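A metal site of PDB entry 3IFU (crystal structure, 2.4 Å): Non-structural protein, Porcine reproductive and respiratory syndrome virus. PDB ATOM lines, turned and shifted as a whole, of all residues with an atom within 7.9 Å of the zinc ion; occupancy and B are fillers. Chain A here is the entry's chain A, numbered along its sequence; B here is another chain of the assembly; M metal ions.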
ATOM      1  N   ARG A   7      26.102   4.505  25.363  1.00  0.00           N
ATOM      2  CA  ARG A   7      25.106   5.482  25.788  1.00  0.00           C
ATOM      3  C   ARG A   7      25.678   6.430  26.847  1.00  0.00           C
ATOM      4  O   ARG A   7      26.867   6.388  27.142  1.00  0.00           O
ATOM      5  CB  ARG A   7      23.903   4.741  26.382  1.00  0.00           C
ATOM      6  CG  ARG A   7      22.547   5.082  25.784  1.00  0.00           C
ATOM      7  CD  ARG A   7      22.362   4.591  24.360  1.00  0.00           C
ATOM      8  NE  ARG A   7      20.978   4.776  23.926  1.00  0.00           N
ATOM      9  CZ  ARG A   7      20.537   4.596  22.689  1.00  0.00           C
ATOM     10  NH1 ARG A   7      21.376   4.217  21.731  1.00  0.00           N
ATOM     11  NH2 ARG A   7      19.252   4.797  22.397  1.00  0.00           N
ATOM     12  N   CYS A   8      24.818   7.263  27.422  1.00  0.00           N
ATOM     13  CA  CYS A   8      25.226   8.190  28.464  1.00  0.00           C
ATOM     14  C   CYS A   8      25.342   7.463  29.795  1.00  0.00           C
ATOM     15  O   CYS A   8      24.484   6.643  30.137  1.00  0.00           O
ATOM     16  CB  CYS A   8      24.197   9.318  28.597  1.00  0.00           C
ATOM     17  SG  CYS A   8      24.213  10.130  30.228  1.00  0.00           S
ATOM     18  N   THR A   9      26.390   7.764  30.552  1.00  0.00           N
ATOM     19  CA  THR A   9      26.608   7.130  31.838  1.00  0.00           C
ATOM     20  C   THR A   9      26.856   8.143  32.943  1.00  0.00           C
ATOM     21  O   THR A   9      27.705   7.939  33.802  1.00  0.00           O
ATOM     22  CB  THR A   9      27.823   6.179  31.811  1.00  0.00           C
ATOM     23  OG1 THR A   9      27.807   5.422  30.596  1.00  0.00           O
ATOM     24  CG2 THR A   9      27.770   5.217  32.987  1.00  0.00           C
ATOM     25  N   CYS A  10      26.112   9.239  32.900  1.00  0.00           N
ATOM     26  CA  CYS A  10      26.231  10.285  33.918  1.00  0.00           C
ATOM     27  C   CYS A  10      25.220   9.987  35.023  1.00  0.00           C
ATOM     28  O   CYS A  10      24.369   9.116  34.866  1.00  0.00           O
ATOM     29  CB  CYS A  10      25.943  11.665  33.316  1.00  0.00           C
ATOM     30  SG  CYS A  10      27.196  12.315  32.194  1.00  0.00           S
ATOM     31  N   THR A  11      25.315  10.709  36.136  1.00  0.00           N
ATOM     32  CA  THR A  11      24.357  10.523  37.211  1.00  0.00           C
ATOM     33  C   THR A  11      22.991  10.884  36.610  1.00  0.00           C
ATOM     34  O   THR A  11      22.864  11.860  35.879  1.00  0.00           O
ATOM     35  CB  THR A  11      24.689  11.444  38.406  1.00  0.00           C
ATOM     36  OG1 THR A  11      24.720  12.810  37.981  1.00  0.00           O
ATOM     37  CG2 THR A  11      26.055  11.084  38.976  1.00  0.00           C
ATOM     38  N   ALA A  14      21.506  14.448  35.674  1.00  0.00           N
ATOM     39  CA  ALA A  14      22.072  15.290  34.634  1.00  0.00           C
ATOM     40  C   ALA A  14      20.936  15.596  33.656  1.00  0.00           C
ATOM     41  O   ALA A  14      20.338  14.681  33.088  1.00  0.00           O
ATOM     42  CB  ALA A  14      23.184  14.554  33.919  1.00  0.00           C
ATOM     43  N   ARG A  15      20.640  16.882  33.461  1.00  0.00           N
ATOM     44  CA  ARG A  15      19.549  17.285  32.567  1.00  0.00           C
ATOM     45  C   ARG A  15      19.583  16.705  31.154  1.00  0.00           C
ATOM     46  O   ARG A  15      20.631  16.322  30.621  1.00  0.00           O
ATOM     47  CB  ARG A  15      19.451  18.808  32.505  1.00  0.00           C
ATOM     48  CG  ARG A  15      19.070  19.417  33.849  1.00  0.00           C
ATOM     49  CD  ARG A  15      18.841  20.900  33.739  1.00  0.00           C
ATOM     50  NE  ARG A  15      18.685  21.533  35.046  1.00  0.00           N
ATOM     51  CZ  ARG A  15      19.687  21.720  35.900  1.00  0.00           C
ATOM     52  NH1 ARG A  15      19.466  22.298  37.065  1.00  0.00           N
ATOM     53  NH2 ARG A  15      20.918  21.342  35.570  1.00  0.00           N
ATOM     54  N   VAL A  16      18.410  16.688  30.544  1.00  0.00           N
ATOM     55  CA  VAL A  16      18.220  16.133  29.222  1.00  0.00           C
ATOM     56  C   VAL A  16      17.609  17.105  28.212  1.00  0.00           C
ATOM     57  O   VAL A  16      16.926  18.067  28.590  1.00  0.00           O
ATOM     58  CB  VAL A  16      17.316  14.871  29.329  1.00  0.00           C
ATOM     59  CG1 VAL A  16      16.708  14.534  27.994  1.00  0.00           C
ATOM     60  CG2 VAL A  16      18.133  13.688  29.851  1.00  0.00           C
ATOM     61  N   TYR A  24      18.918  13.282  24.580  1.00  0.00           N
ATOM     62  CA  TYR A  24      20.367  13.355  24.803  1.00  0.00           C
ATOM     63  C   TYR A  24      20.660  13.960  26.163  1.00  0.00           C
ATOM     64  O   TYR A  24      19.837  14.684  26.726  1.00  0.00           O
ATOM     65  CB  TYR A  24      21.067  14.229  23.748  1.00  0.00           C
ATOM     66  CG  TYR A  24      21.094  13.700  22.324  1.00  0.00           C
ATOM     67  CD1 TYR A  24      20.083  14.014  21.412  1.00  0.00           C
ATOM     68  CD2 TYR A  24      22.163  12.913  21.878  1.00  0.00           C
ATOM     69  CE1 TYR A  24      20.146  13.571  20.100  1.00  0.00           C
ATOM     70  CE2 TYR A  24      22.225  12.470  20.566  1.00  0.00           C
ATOM     71  CZ  TYR A  24      21.226  12.794  19.680  1.00  0.00           C
ATOM     72  OH  TYR A  24      21.317  12.361  18.378  1.00  0.00           O
ATOM     73  N   CYS A  25      21.844  13.680  26.681  1.00  0.00           N
ATOM     74  CA  CYS A  25      22.268  14.198  27.968  1.00  0.00           C
ATOM     75  C   CYS A  25      22.895  15.581  27.778  1.00  0.00           C
ATOM     76  O   CYS A  25      23.688  15.790  26.868  1.00  0.00           O
ATOM     77  CB  CYS A  25      23.289  13.273  28.605  1.00  0.00           C
ATOM     78  SG  CYS A  25      24.108  13.989  30.041  1.00  0.00           S
ATOM     79  N   THR A  26      22.516  16.508  28.645  1.00  0.00           N
ATOM     80  CA  THR A  26      23.029  17.864  28.593  1.00  0.00           C
ATOM     81  C   THR A  26      24.524  17.934  28.928  1.00  0.00           C
ATOM     82  O   THR A  26      25.236  18.817  28.462  1.00  0.00           O
ATOM     83  CB  THR A  26      22.237  18.754  29.577  1.00  0.00           C
ATOM     84  OG1 THR A  26      20.969  19.085  28.999  1.00  0.00           O
ATOM     85  CG2 THR A  26      22.984  20.029  29.882  1.00  0.00           C
ATOM     86  N   ARG A  27      24.998  16.979  29.730  1.00  0.00           N
ATOM     87  CA  ARG A  27      26.397  16.935  30.153  1.00  0.00           C
ATOM     88  C   ARG A  27      27.418  16.378  29.157  1.00  0.00           C
ATOM     89  O   ARG A  27      28.438  17.035  28.898  1.00  0.00           O
ATOM     90  CB  ARG A  27      26.520  16.148  31.463  1.00  0.00           C
ATOM     91  CG  ARG A  27      26.292  16.953  32.709  1.00  0.00           C
ATOM     92  CD  ARG A  27      27.418  16.685  33.716  1.00  0.00           C
ATOM     93  NE  ARG A  27      27.146  15.590  34.640  1.00  0.00           N
ATOM     94  CZ  ARG A  27      26.218  15.628  35.606  1.00  0.00           C
ATOM     95  NH1 ARG A  27      25.457  16.707  35.759  1.00  0.00           N
ATOM     96  NH2 ARG A  27      26.063  14.597  36.414  1.00  0.00           N
ATOM     97  N   CYS A  28      27.172  15.183  28.641  1.00  0.00           N
ATOM     98  CA  CYS A  28      28.113  14.533  27.720  1.00  0.00           C
ATOM     99  C   CYS A  28      27.658  14.451  26.258  1.00  0.00           C
ATOM    100  O   CYS A  28      28.391  13.937  25.416  1.00  0.00           O
ATOM    101  CB  CYS A  28      28.423  13.107  28.200  1.00  0.00           C
ATOM    102  SG  CYS A  28      27.019  11.979  28.102  1.00  0.00           S
ATOM    103  N   LEU A  29      26.455  14.942  25.975  1.00  0.00           N
ATOM    104  CA  LEU A  29      25.921  14.947  24.615  1.00  0.00           C
ATOM    105  C   LEU A  29      25.747  13.556  24.011  1.00  0.00           C
ATOM    106  O   LEU A  29      25.683  13.399  22.792  1.00  0.00           O
ATOM    107  CB  LEU A  29      26.829  15.796  23.718  1.00  0.00           C
ATOM    108  CG  LEU A  29      27.146  17.180  24.278  1.00  0.00           C
ATOM    109  CD1 LEU A  29      28.280  17.846  23.518  1.00  0.00           C
ATOM    110  CD2 LEU A  29      25.882  18.012  24.231  1.00  0.00           C
ATOM    111  N   SER A  30      25.670  12.534  24.869  1.00  0.00           N
ATOM    112  CA  SER A  30      25.481  11.168  24.398  1.00  0.00           C
ATOM    113  C   SER A  30      24.021  10.790  24.585  1.00  0.00           C
ATOM    114  O   SER A  30      23.360  11.303  25.495  1.00  0.00           O
ATOM    115  CB  SER A  30      26.372  10.217  25.190  1.00  0.00           C
ATOM    116  OG  SER A  30      27.736  10.572  25.063  1.00  0.00           O
ATOM    117  N   ALA A  31      23.533   9.896  23.739  1.00  0.00           N
ATOM    118  CA  ALA A  31      22.143   9.442  23.820  1.00  0.00           C
ATOM    119  C   ALA A  31      21.804   8.929  25.210  1.00  0.00           C
ATOM    120  O   ALA A  31      22.624   8.262  25.848  1.00  0.00           O
ATOM    121  CB  ALA A  31      21.891   8.346  22.785  1.00  0.00           C
ATOM    122  N   ARG A  32      20.606   9.233  25.686  1.00  0.00           N
ATOM    123  CA  ARG A  32      20.167   8.803  27.000  1.00  0.00           C
ATOM    124  C   ARG A  32      19.173   7.645  26.973  1.00  0.00           C
ATOM    125  O   ARG A  32      18.133   7.720  26.317  1.00  0.00           O
ATOM    126  CB  ARG A  32      19.541   9.972  27.757  1.00  0.00           C
ATOM    127  CG  ARG A  32      20.435  10.531  28.830  1.00  0.00           C
ATOM    128  CD  ARG A  32      20.325   9.734  30.110  1.00  0.00           C
ATOM    129  NE  ARG A  32      19.709  10.532  31.164  1.00  0.00           N
ATOM    130  CZ  ARG A  32      20.247  11.618  31.695  1.00  0.00           C
ATOM    131  NH1 ARG A  32      21.429  12.052  31.273  1.00  0.00           N
ATOM    132  NH2 ARG A  32      19.611  12.279  32.652  1.00  0.00           N
ATOM    133  N   PRO B 165      32.028  13.105  23.452  1.00  0.00           N
ATOM    134  CA  PRO B 165      32.648  12.292  24.503  1.00  0.00           C
ATOM    135  C   PRO B 165      33.675  11.298  23.960  1.00  0.00           C
ATOM    136  O   PRO B 165      34.657  10.982  24.628  1.00  0.00           O
ATOM    137  CB  PRO B 165      31.444  11.589  25.130  1.00  0.00           C
ATOM    138  CG  PRO B 165      30.627  11.285  23.934  1.00  0.00           C
ATOM    139  CD  PRO B 165      30.675  12.614  23.163  1.00  0.00           C
HETATM  140 ZN    ZN M   1      25.728  12.165  30.177  1.00  0.00          ZN
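The zinc ion is bound by the side-chain sulfur (SG) of Cys 25 (2.4 Å), the side-chain sulfur (SG) of Cys 28 (2.5 Å), the side-chain sulfur (SG) of Cys 10 (2.5 Å) and the side-chain sulfur (SG) of Cys 8 (2.5 Å).
O of Cys 28 is in hydrogen-bond range of OG of Ser 30 (3.4 Å).
The side-chain sulfur of Cys 25 lies close to the backbone NH of Arg 27 (3.1 Å).
N of Cys 25 lies within hydrogen-bond range of O of Ser 30 (3.1 Å).
The guanidinium group (NH1) of Arg 32 sits close to the side-chain sulfur (SG) of Cys 8, at 3.5 Å.
The backbone NH (N) of Cys 8 lies within hydrogen-bond range of the backbone carbonyl oxygen (O) of Ala 31 (2.9 Å).
The side-chain sulfur (SG) of Cys 25 sits close to the guanidinium group (NH1) of Arg 32.
Along chain A the residues within 4 Å of the zinc ion span positions 8 to 28.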
